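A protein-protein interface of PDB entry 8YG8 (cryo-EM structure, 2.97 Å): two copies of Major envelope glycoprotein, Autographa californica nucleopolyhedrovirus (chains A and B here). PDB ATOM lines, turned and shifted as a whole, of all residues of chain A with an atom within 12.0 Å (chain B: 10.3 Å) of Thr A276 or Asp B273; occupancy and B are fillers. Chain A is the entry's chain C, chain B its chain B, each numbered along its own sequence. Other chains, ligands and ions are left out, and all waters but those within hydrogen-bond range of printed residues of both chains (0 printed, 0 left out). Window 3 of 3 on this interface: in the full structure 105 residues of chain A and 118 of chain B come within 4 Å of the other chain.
The side-chain carboxylate (OD1) of Asp A279 lies within salt-bridge range of the guanidinium group (NH2) of Arg B266 (3.8 Å).
OH of Tyr B269 is in hydrogen-bond range of OE2 of Glu A285, at 2.8 Å.
The backbone carbonyl oxygen (O) of Ala A275 is in hydrogen-bond range of the backbone NH (N) of Ala B275 (2.9 Å).
The side-chain carboxylate of Glu A285 lies close to the side-chain amino group of Lys B268 (2.3 Å).
O of Lys B268 is in hydrogen-bond range of OG1 of Thr B270.
The side-chain hydroxyl of Thr B276 is in hydrogen-bond range of the side-chain carboxylate of Asp B279, at 2.9 Å.
The side-chain hydroxyl (OG1) of Thr A276 is in hydrogen-bond range of the side-chain carboxylate (OD2) of Asp A279 (3.1 Å).
Among the printed residues, merely in contact across the chains: Asp A279 with Ala B267 (3.2 Å), Thr A276 with Asp B273 (3.3 Å), Met A281 with Glu B271 (3.3 Å), His A282 with Trp B261 (3.4 Å), Gly A278 with Tyr B269 (3.4 Å), Gln A284 with Ile B283 (3.4 Å), Lys A277 with Asp B273 (3.6 Å), Asp A279 with Trp B261 (3.6 Å), Ile A283 with Trp B261 (3.6 Å), Ala A275 with Asp B273 (3.6 Å), Met A281 with Tyr B269 (3.7 Å), Ala A275 with Thr B274 (3.7 Å), Leu A280 with Ile B283 (3.7 Å), Leu A280 with Asp B279 (3.8 Å), His A282 with Lys B268 (3.9 Å) and Lys A277 with Glu B271 (3.9 Å).
Gly A272 touches none of the printed residues of chain B.
Printed residues of chain B within 4 Å of Ala A275: Asp B273, Thr B274 and Ala B275.
Printed residues of chain B within 4 Å of Thr A276: Asp B273.
Printed residues of chain B within 4 Å of Lys A277: Glu B271 (3.9 Å) and Asp B273 (3.6 Å).
Printed residues of chain B within 4 Å of Gly A278: Tyr B269 (3.4 Å).
Of the printed residues of chain B, Gln A284 touches Ile B283.
Of the printed residues of chain B, Glu A285 touches Lys B268 (2.3 Å) and Tyr B269 (2.8 Å).
Ala B267 touches just one residue of chain A: Asp A279 (3.2 Å).
Printed residues of chain A within 4 Å of Tyr B269: Gly A278 (3.4 Å), Met A281 (3.7 Å) and Glu A285 (2.8 Å).
Of chain A, only Lys A277 (3.9 Å) and Met A281 (3.3 Å) come within 4 Å of Glu B271.
No residue of chain A comes within 4 Å of Gly B272.
Printed residues of chain A within 4 Å of Asp B273: Ala A275, Thr A276 and Lys A277.
Of chain A, only Ala A275 comes within 4 Å of Thr B274.
Ala B275 touches just one residue of chain A: Ala A275 (2.9 Å).
The nearest residue of chain B that does not touch Thr A276 is Glu B271 (4.02 Å).
Of the 18 printed residues of chain B, 11 touch a printed residue of chain A.
Hydrophobic or aromatic side chains of chain B within 4 Å of the printed part of chain A: Trp B261, Ala B267, Tyr B269, Ala B275 and Ile B283.
Of the 15 printed residues of chain A, 11 touch a printed residue of chain B.
Printed residues of chain A that touch a printed residue of chain B: Ala A275, Thr A276, Lys A277, Gly A278, Asp A279, Leu A280, Met A281, His A282, Ile A283, Gln A284 and Glu A285.
Hydrophobic or aromatic side chains of chain A that line the printed part of chain B: Ala A275, Leu A280, Met A281, His A282 and Ile A283.
Among the printed residues, Asp or Glu carboxylates within 4 Å of a Lys or Arg side-chain nitrogen of the other chain: Asp A279 with Arg B266 and Glu A285 with Lys B268.
Ala A275 touches Thr B274, but with the chains exchanged Thr A274 does not touch Ala B275 (5.2 Å).
Ala A275 touches its own counterpart, Ala B275.
Lys A277 touches Glu B271, but with the chains exchanged Glu A271 does not touch Lys B277 (10.1 Å).
Leu A280 touches Asp B279, but with the chains exchanged Asp A279 does not touch Leu B280 (8.4 Å).
10 positions are printed for both chains.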
ATOM      1  N   GLU A 271      -2.009  19.630  -0.973  1.00  0.00           N
ATOM      2  CA  GLU A 271      -2.803  20.086   0.165  1.00  0.00           C
ATOM      3  C   GLU A 271      -1.842  20.767   1.134  1.00  0.00           C
ATOM      4  O   GLU A 271      -1.033  20.099   1.786  1.00  0.00           O
ATOM      5  CB  GLU A 271      -3.542  18.927   0.821  1.00  0.00           C
ATOM      6  CG  GLU A 271      -4.865  18.594   0.156  1.00  0.00           C
ATOM      7  CD  GLU A 271      -5.416  17.257   0.597  1.00  0.00           C
ATOM      8  OE1 GLU A 271      -4.673  16.496   1.251  1.00  0.00           O
ATOM      9  OE2 GLU A 271      -6.591  16.964   0.290  1.00  0.00           O
ATOM     10  N   GLY A 272      -1.925  22.093   1.222  1.00  0.00           N
ATOM     11  CA  GLY A 272      -0.996  22.854   2.033  1.00  0.00           C
ATOM     12  C   GLY A 272      -1.111  22.407   3.476  1.00  0.00           C
ATOM     13  O   GLY A 272      -2.174  22.528   4.090  1.00  0.00           O
ATOM     14  N   ASP A 273      -0.014  21.901   4.024  1.00  0.00           N
ATOM     15  CA  ASP A 273       0.056  21.450   5.409  1.00  0.00           C
ATOM     16  C   ASP A 273       1.511  21.091   5.677  1.00  0.00           C
ATOM     17  O   ASP A 273       2.347  21.088   4.769  1.00  0.00           O
ATOM     18  CB  ASP A 273      -0.882  20.294   5.761  1.00  0.00           C
ATOM     19  CG  ASP A 273      -2.256  20.767   6.181  1.00  0.00           C
ATOM     20  OD1 ASP A 273      -2.335  21.735   6.965  1.00  0.00           O
ATOM     21  OD2 ASP A 273      -3.255  20.180   5.720  1.00  0.00           O
ATOM     22  N   THR A 274       1.809  20.780   6.934  1.00  0.00           N
ATOM     23  CA  THR A 274       3.160  20.441   7.357  1.00  0.00           C
ATOM     24  C   THR A 274       3.217  18.967   7.721  1.00  0.00           C
ATOM     25  O   THR A 274       2.393  18.485   8.505  1.00  0.00           O
ATOM     26  CB  THR A 274       3.597  21.297   8.547  1.00  0.00           C
ATOM     27  OG1 THR A 274       3.614  22.676   8.163  1.00  0.00           O
ATOM     28  CG2 THR A 274       4.986  20.890   9.011  1.00  0.00           C
ATOM     29  N   ALA A 275       4.182  18.257   7.148  1.00  0.00           N
ATOM     30  CA  ALA A 275       4.365  16.845   7.431  1.00  0.00           C
ATOM     31  C   ALA A 275       5.242  16.658   8.661  1.00  0.00           C
ATOM     32  O   ALA A 275       6.140  17.458   8.938  1.00  0.00           O
ATOM     33  CB  ALA A 275       4.986  16.127   6.233  1.00  0.00           C
ATOM     34  N   THR A 276       4.972  15.588   9.398  1.00  0.00           N
ATOM     35  CA  THR A 276       5.706  15.249  10.606  1.00  0.00           C
ATOM     36  C   THR A 276       6.407  13.910  10.419  1.00  0.00           C
ATOM     37  O   THR A 276       6.220  13.216   9.417  1.00  0.00           O
ATOM     38  CB  THR A 276       4.775  15.196  11.822  1.00  0.00           C
ATOM     39  OG1 THR A 276       3.777  14.188  11.614  1.00  0.00           O
ATOM     40  CG2 THR A 276       4.093  16.536  12.023  1.00  0.00           C
ATOM     41  N   LYS A 277       7.229  13.551  11.406  1.00  0.00           N
ATOM     42  CA  LYS A 277       7.976  12.301  11.319  1.00  0.00           C
ATOM     43  C   LYS A 277       7.051  11.091  11.373  1.00  0.00           C
ATOM     44  O   LYS A 277       7.268  10.108  10.654  1.00  0.00           O
ATOM     45  CB  LYS A 277       9.014  12.235  12.437  1.00  0.00           C
ATOM     46  CG  LYS A 277       9.855  13.491  12.567  1.00  0.00           C
ATOM     47  CD  LYS A 277      11.108  13.410  11.716  1.00  0.00           C
ATOM     48  CE  LYS A 277      12.109  14.482  12.114  1.00  0.00           C
ATOM     49  NZ  LYS A 277      13.306  14.489  11.228  1.00  0.00           N
ATOM     50  N   GLY A 278       6.011  11.150  12.209  1.00  0.00           N
ATOM     51  CA  GLY A 278       5.150   9.991  12.398  1.00  0.00           C
ATOM     52  C   GLY A 278       4.487   9.528  11.115  1.00  0.00           C
ATOM     53  O   GLY A 278       4.340   8.325  10.878  1.00  0.00           O
ATOM     54  N   ASP A 279       4.076  10.475  10.269  1.00  0.00           N
ATOM     55  CA  ASP A 279       3.497  10.110   8.982  1.00  0.00           C
ATOM     56  C   ASP A 279       4.501   9.341   8.135  1.00  0.00           C
ATOM     57  O   ASP A 279       4.158   8.329   7.506  1.00  0.00           O
ATOM     58  CB  ASP A 279       3.034  11.369   8.249  1.00  0.00           C
ATOM     59  CG  ASP A 279       2.245  12.304   9.142  1.00  0.00           C
ATOM     60  OD1 ASP A 279       1.508  11.811  10.020  1.00  0.00           O
ATOM     61  OD2 ASP A 279       2.365  13.534   8.969  1.00  0.00           O
ATOM     62  N   LEU A 280       5.751   9.804   8.117  1.00  0.00           N
ATOM     63  CA  LEU A 280       6.788   9.127   7.349  1.00  0.00           C
ATOM     64  C   LEU A 280       7.032   7.722   7.887  1.00  0.00           C
ATOM     65  O   LEU A 280       7.196   6.769   7.115  1.00  0.00           O
ATOM     66  CB  LEU A 280       8.066   9.962   7.374  1.00  0.00           C
ATOM     67  CG  LEU A 280       9.173   9.579   6.395  1.00  0.00           C
ATOM     68  CD1 LEU A 280       8.653   9.624   4.972  1.00  0.00           C
ATOM     69  CD2 LEU A 280      10.346  10.523   6.555  1.00  0.00           C
ATOM     70  N   MET A 281       7.047   7.572   9.215  1.00  0.00           N
ATOM     71  CA  MET A 281       7.197   6.245   9.805  1.00  0.00           C
ATOM     72  C   MET A 281       6.056   5.323   9.401  1.00  0.00           C
ATOM     73  O   MET A 281       6.287   4.153   9.075  1.00  0.00           O
ATOM     74  CB  MET A 281       7.260   6.341  11.327  1.00  0.00           C
ATOM     75  CG  MET A 281       8.171   7.425  11.850  1.00  0.00           C
ATOM     76  SD  MET A 281       8.267   7.425  13.646  1.00  0.00           S
ATOM     77  CE  MET A 281       9.762   8.374  13.888  1.00  0.00           C
ATOM     78  N   HIS A 282       4.824   5.835   9.424  1.00  0.00           N
ATOM     79  CA  HIS A 282       3.667   5.028   9.050  1.00  0.00           C
ATOM     80  C   HIS A 282       3.774   4.560   7.604  1.00  0.00           C
ATOM     81  O   HIS A 282       3.558   3.376   7.295  1.00  0.00           O
ATOM     82  CB  HIS A 282       2.395   5.849   9.268  1.00  0.00           C
ATOM     83  CG  HIS A 282       1.134   5.049   9.208  1.00  0.00           C
ATOM     84  ND1 HIS A 282       0.211   5.044  10.231  1.00  0.00           N
ATOM     85  CD2 HIS A 282       0.639   4.231   8.251  1.00  0.00           C
ATOM     86  CE1 HIS A 282      -0.798   4.258   9.906  1.00  0.00           C
ATOM     87  NE2 HIS A 282      -0.564   3.752   8.710  1.00  0.00           N
ATOM     88  N   ILE A 283       4.124   5.481   6.701  1.00  0.00           N
ATOM     89  CA  ILE A 283       4.269   5.128   5.291  1.00  0.00           C
ATOM     90  C   ILE A 283       5.353   4.071   5.117  1.00  0.00           C
ATOM     91  O   ILE A 283       5.173   3.080   4.391  1.00  0.00           O
ATOM     92  CB  ILE A 283       4.569   6.388   4.460  1.00  0.00           C
ATOM     93  CG1 ILE A 283       3.437   7.406   4.596  1.00  0.00           C
ATOM     94  CG2 ILE A 283       4.773   6.030   3.003  1.00  0.00           C
ATOM     95  CD1 ILE A 283       2.187   7.028   3.854  1.00  0.00           C
ATOM     96  N   GLN A 284       6.492   4.264   5.788  1.00  0.00           N
ATOM     97  CA  GLN A 284       7.598   3.322   5.672  1.00  0.00           C
ATOM     98  C   GLN A 284       7.191   1.933   6.142  1.00  0.00           C
ATOM     99  O   GLN A 284       7.504   0.929   5.490  1.00  0.00           O
ATOM    100  CB  GLN A 284       8.791   3.838   6.474  1.00  0.00           C
ATOM    101  CG  GLN A 284      10.124   3.240   6.080  1.00  0.00           C
ATOM    102  CD  GLN A 284      11.226   3.609   7.049  1.00  0.00           C
ATOM    103  OE1 GLN A 284      11.002   3.707   8.253  1.00  0.00           O
ATOM    104  NE2 GLN A 284      12.427   3.822   6.525  1.00  0.00           N
ATOM    105  N   GLU A 285       6.481   1.858   7.270  1.00  0.00           N
ATOM    106  CA  GLU A 285       6.050   0.564   7.789  1.00  0.00           C
ATOM    107  C   GLU A 285       5.100  -0.129   6.820  1.00  0.00           C
ATOM    108  O   GLU A 285       5.214  -1.342   6.581  1.00  0.00           O
ATOM    109  CB  GLU A 285       5.393   0.756   9.153  1.00  0.00           C
ATOM    110  CG  GLU A 285       5.536  -0.424  10.088  1.00  0.00           C
ATOM    111  CD  GLU A 285       5.163  -0.074  11.512  1.00  0.00           C
ATOM    112  OE1 GLU A 285       3.956   0.060  11.797  1.00  0.00           O
ATOM    113  OE2 GLU A 285       6.079   0.076  12.346  1.00  0.00           O
ATOM    114  N   TRP B 261      -2.314   4.557   5.588  1.00  0.00           N
ATOM    115  CA  TRP B 261      -2.156   5.946   5.990  1.00  0.00           C
ATOM    116  C   TRP B 261      -2.951   6.858   5.071  1.00  0.00           C
ATOM    117  O   TRP B 261      -3.009   6.643   3.857  1.00  0.00           O
ATOM    118  CB  TRP B 261      -0.684   6.354   5.969  1.00  0.00           C
ATOM    119  CG  TRP B 261      -0.451   7.766   6.402  1.00  0.00           C
ATOM    120  CD1 TRP B 261      -0.164   8.196   7.660  1.00  0.00           C
ATOM    121  CD2 TRP B 261      -0.484   8.936   5.575  1.00  0.00           C
ATOM    122  NE1 TRP B 261      -0.016   9.561   7.672  1.00  0.00           N
ATOM    123  CE2 TRP B 261      -0.207  10.039   6.404  1.00  0.00           C
ATOM    124  CE3 TRP B 261      -0.720   9.156   4.216  1.00  0.00           C
ATOM    125  CZ2 TRP B 261      -0.161  11.343   5.919  1.00  0.00           C
ATOM    126  CZ3 TRP B 261      -0.673  10.451   3.737  1.00  0.00           C
ATOM    127  CH2 TRP B 261      -0.396  11.527   4.586  1.00  0.00           C
ATOM    128  N   ARG B 262      -3.561   7.882   5.659  1.00  0.00           N
ATOM    129  CA  ARG B 262      -4.279   8.886   4.893  1.00  0.00           C
ATOM    130  C   ARG B 262      -4.289  10.185   5.682  1.00  0.00           C
ATOM    131  O   ARG B 262      -4.221  10.187   6.913  1.00  0.00           O
ATOM    132  CB  ARG B 262      -5.709   8.438   4.574  1.00  0.00           C
ATOM    133  CG  ARG B 262      -6.544   8.121   5.801  1.00  0.00           C
ATOM    134  CD  ARG B 262      -7.824   7.380   5.442  1.00  0.00           C
ATOM    135  NE  ARG B 262      -7.565   6.097   4.800  1.00  0.00           N
ATOM    136  CZ  ARG B 262      -7.652   5.881   3.495  1.00  0.00           C
ATOM    137  NH1 ARG B 262      -7.991   6.846   2.655  1.00  0.00           N
ATOM    138  NH2 ARG B 262      -7.392   4.666   3.019  1.00  0.00           N
ATOM    139  N   VAL B 265      -6.443  12.015   9.115  1.00  0.00           N
ATOM    140  CA  VAL B 265      -6.557  10.929  10.082  1.00  0.00           C
ATOM    141  C   VAL B 265      -5.241  10.833  10.840  1.00  0.00           C
ATOM    142  O   VAL B 265      -4.165  10.958  10.244  1.00  0.00           O
ATOM    143  CB  VAL B 265      -6.895   9.585   9.405  1.00  0.00           C
ATOM    144  CG1 VAL B 265      -6.956   8.468  10.432  1.00  0.00           C
ATOM    145  CG2 VAL B 265      -8.216   9.679   8.656  1.00  0.00           C
ATOM    146  N   ARG B 266      -5.325  10.625  12.152  1.00  0.00           N
ATOM    147  CA  ARG B 266      -4.133  10.493  12.977  1.00  0.00           C
ATOM    148  C   ARG B 266      -3.291   9.309  12.511  1.00  0.00           C
ATOM    149  O   ARG B 266      -3.811   8.251  12.148  1.00  0.00           O
ATOM    150  CB  ARG B 266      -4.524  10.316  14.445  1.00  0.00           C
ATOM    151  CG  ARG B 266      -3.361  10.128  15.407  1.00  0.00           C
ATOM    152  CD  ARG B 266      -2.562  11.410  15.582  1.00  0.00           C
ATOM    153  NE  ARG B 266      -1.542  11.578  14.553  1.00  0.00           N
ATOM    154  CZ  ARG B 266      -0.821  12.678  14.385  1.00  0.00           C
ATOM    155  NH1 ARG B 266      -0.978  13.733  15.168  1.00  0.00           N
ATOM    156  NH2 ARG B 266       0.079  12.719  13.407  1.00  0.00           N
ATOM    157  N   ALA B 267      -1.975   9.497  12.520  1.00  0.00           N
ATOM    158  CA  ALA B 267      -1.031   8.527  11.966  1.00  0.00           C
ATOM    159  C   ALA B 267      -0.222   7.902  13.099  1.00  0.00           C
ATOM    160  O   ALA B 267       0.883   8.350  13.403  1.00  0.00           O
ATOM    161  CB  ALA B 267      -0.122   9.191  10.942  1.00  0.00           C
ATOM    162  N   LYS B 268      -0.782   6.844  13.695  1.00  0.00           N
ATOM    163  CA  LYS B 268      -0.180   6.010  14.737  1.00  0.00           C
ATOM    164  C   LYS B 268       0.981   6.651  15.491  1.00  0.00           C
ATOM    165  O   LYS B 268       0.845   7.003  16.667  1.00  0.00           O
ATOM    166  CB  LYS B 268       0.281   4.684  14.127  1.00  0.00           C
ATOM    167  CG  LYS B 268       0.825   3.695  15.140  1.00  0.00           C
ATOM    168  CD  LYS B 268       0.866   2.287  14.568  1.00  0.00           C
ATOM    169  CE  LYS B 268       1.953   2.144  13.521  1.00  0.00           C
ATOM    170  NZ  LYS B 268       2.156   0.722  13.130  1.00  0.00           N
ATOM    171  N   TYR B 269       2.126   6.799  14.828  1.00  0.00           N
ATOM    172  CA  TYR B 269       3.300   7.371  15.476  1.00  0.00           C
ATOM    173  C   TYR B 269       3.081   8.850  15.762  1.00  0.00           C
ATOM    174  O   TYR B 269       2.821   9.636  14.846  1.00  0.00           O
ATOM    175  CB  TYR B 269       4.531   7.178  14.594  1.00  0.00           C
ATOM    176  CG  TYR B 269       5.046   5.759  14.547  1.00  0.00           C
ATOM    177  CD1 TYR B 269       5.928   5.289  15.510  1.00  0.00           C
ATOM    178  CD2 TYR B 269       4.659   4.893  13.536  1.00  0.00           C
ATOM    179  CE1 TYR B 269       6.404   3.994  15.469  1.00  0.00           C
ATOM    180  CE2 TYR B 269       5.130   3.597  13.487  1.00  0.00           C
ATOM    181  CZ  TYR B 269       6.001   3.153  14.456  1.00  0.00           C
ATOM    182  OH  TYR B 269       6.473   1.862  14.411  1.00  0.00           O
ATOM    183  N   THR B 270       3.203   9.231  17.029  1.00  0.00           N
ATOM    184  CA  THR B 270       2.980  10.604  17.463  1.00  0.00           C
ATOM    185  C   THR B 270       4.309  11.225  17.869  1.00  0.00           C
ATOM    186  O   THR B 270       4.745  11.069  19.015  1.00  0.00           O
ATOM    187  CB  THR B 270       1.990  10.656  18.626  1.00  0.00           C
ATOM    188  OG1 THR B 270       0.862   9.825  18.330  1.00  0.00           O
ATOM    189  CG2 THR B 270       1.514  12.081  18.854  1.00  0.00           C
ATOM    190  N   GLU B 271       4.945  11.930  16.932  1.00  0.00           N
ATOM    191  CA  GLU B 271       6.183  12.657  17.218  1.00  0.00           C
ATOM    192  C   GLU B 271       6.128  13.964  16.434  1.00  0.00           C
ATOM    193  O   GLU B 271       6.496  13.999  15.257  1.00  0.00           O
ATOM    194  CB  GLU B 271       7.412  11.837  16.852  1.00  0.00           C
ATOM    195  CG  GLU B 271       7.647  10.626  17.739  1.00  0.00           C
ATOM    196  CD  GLU B 271       8.925   9.892  17.394  1.00  0.00           C
ATOM    197  OE1 GLU B 271       9.692  10.398  16.548  1.00  0.00           O
ATOM    198  OE2 GLU B 271       9.164   8.809  17.969  1.00  0.00           O
ATOM    199  N   GLY B 272       5.674  15.027  17.092  1.00  0.00           N
ATOM    200  CA  GLY B 272       5.539  16.314  16.441  1.00  0.00           C
ATOM    201  C   GLY B 272       6.863  16.936  16.053  1.00  0.00           C
ATOM    202  O   GLY B 272       7.653  17.323  16.917  1.00  0.00           O
ATOM    203  N   ASP B 273       7.110  17.042  14.752  1.00  0.00           N
ATOM    204  CA  ASP B 273       8.329  17.641  14.223  1.00  0.00           C
ATOM    205  C   ASP B 273       8.026  18.161  12.822  1.00  0.00           C
ATOM    206  O   ASP B 273       6.863  18.265  12.420  1.00  0.00           O
ATOM    207  CB  ASP B 273       9.484  16.635  14.227  1.00  0.00           C
ATOM    208  CG  ASP B 273      10.211  16.587  15.554  1.00  0.00           C
ATOM    209  OD1 ASP B 273      10.343  17.649  16.198  1.00  0.00           O
ATOM    210  OD2 ASP B 273      10.648  15.489  15.955  1.00  0.00           O
ATOM    211  N   THR B 274       9.076  18.492  12.076  1.00  0.00           N
ATOM    212  CA  THR B 274       8.943  19.032  10.729  1.00  0.00           C
ATOM    213  C   THR B 274       9.724  18.157   9.763  1.00  0.00           C
ATOM    214  O   THR B 274      10.924  17.933   9.955  1.00  0.00           O
ATOM    215  CB  THR B 274       9.441  20.476  10.665  1.00  0.00           C
ATOM    216  OG1 THR B 274       8.773  21.254  11.665  1.00  0.00           O
ATOM    217  CG2 THR B 274       9.161  21.071   9.296  1.00  0.00           C
ATOM    218  N   ALA B 275       9.047  17.666   8.731  1.00  0.00           N
ATOM    219  CA  ALA B 275       9.690  16.834   7.729  1.00  0.00           C
ATOM    220  C   ALA B 275      10.350  17.692   6.656  1.00  0.00           C
ATOM    221  O   ALA B 275       9.817  18.723   6.238  1.00  0.00           O
ATOM    222  CB  ALA B 275       8.678  15.885   7.089  1.00  0.00           C
ATOM    223  N   THR B 276      11.523  17.253   6.212  1.00  0.00           N
ATOM    224  CA  THR B 276      12.279  17.935   5.176  1.00  0.00           C
ATOM    225  C   THR B 276      12.329  17.075   3.920  1.00  0.00           C
ATOM    226  O   THR B 276      12.096  15.864   3.960  1.00  0.00           O
ATOM    227  CB  THR B 276      13.704  18.255   5.641  1.00  0.00           C
ATOM    228  OG1 THR B 276      14.399  17.036   5.930  1.00  0.00           O
ATOM    229  CG2 THR B 276      13.672  19.120   6.886  1.00  0.00           C
ATOM    230  N   LYS B 277      12.642  17.725   2.797  1.00  0.00           N
ATOM    231  CA  LYS B 277      12.668  17.025   1.516  1.00  0.00           C
ATOM    232  C   LYS B 277      13.747  15.949   1.492  1.00  0.00           C
ATOM    233  O   LYS B 277      13.611  14.936   0.794  1.00  0.00           O
ATOM    234  CB  LYS B 277      12.881  18.027   0.384  1.00  0.00           C
ATOM    235  CG  LYS B 277      11.919  19.202   0.414  1.00  0.00           C
ATOM    236  CD  LYS B 277      10.632  18.896  -0.331  1.00  0.00           C
ATOM    237  CE  LYS B 277       9.885  20.176  -0.672  1.00  0.00           C
ATOM    238  NZ  LYS B 277       8.561  19.905  -1.294  1.00  0.00           N
ATOM    239  N   ASP B 279      14.518  13.864   3.840  1.00  0.00           N
ATOM    240  CA  ASP B 279      13.942  12.633   4.368  1.00  0.00           C
ATOM    241  C   ASP B 279      13.113  11.921   3.307  1.00  0.00           C
ATOM    242  O   ASP B 279      13.187  10.691   3.167  1.00  0.00           O
ATOM    243  CB  ASP B 279      13.092  12.949   5.597  1.00  0.00           C
ATOM    244  CG  ASP B 279      13.842  13.768   6.627  1.00  0.00           C
ATOM    245  OD1 ASP B 279      15.046  13.515   6.829  1.00  0.00           O
ATOM    246  OD2 ASP B 279      13.231  14.675   7.228  1.00  0.00           O
ATOM    247  N   LEU B 280      12.319  12.680   2.550  1.00  0.00           N
ATOM    248  CA  LEU B 280      11.526  12.094   1.476  1.00  0.00           C
ATOM    249  C   LEU B 280      12.424  11.422   0.447  1.00  0.00           C
ATOM    250  O   LEU B 280      12.166  10.290   0.020  1.00  0.00           O
ATOM    251  CB  LEU B 280      10.667  13.172   0.814  1.00  0.00           C
ATOM    252  CG  LEU B 280       9.253  13.418   1.342  1.00  0.00           C
ATOM    253  CD1 LEU B 280       8.382  12.197   1.117  1.00  0.00           C
ATOM    254  CD2 LEU B 280       9.268  13.812   2.810  1.00  0.00           C
ATOM    255  N   ILE B 283      13.906   8.123   1.898  1.00  0.00           N
ATOM    256  CA  ILE B 283      12.920   7.047   1.888  1.00  0.00           C
ATOM    257  C   ILE B 283      12.720   6.527   0.470  1.00  0.00           C
ATOM    258  O   ILE B 283      12.661   5.309   0.235  1.00  0.00           O
ATOM    259  CB  ILE B 283      11.599   7.544   2.505  1.00  0.00           C
ATOM    260  CG1 ILE B 283      11.813   7.961   3.959  1.00  0.00           C
ATOM    261  CG2 ILE B 283      10.536   6.472   2.432  1.00  0.00           C
ATOM    262  CD1 ILE B 283      12.132   6.813   4.879  1.00  0.00           C
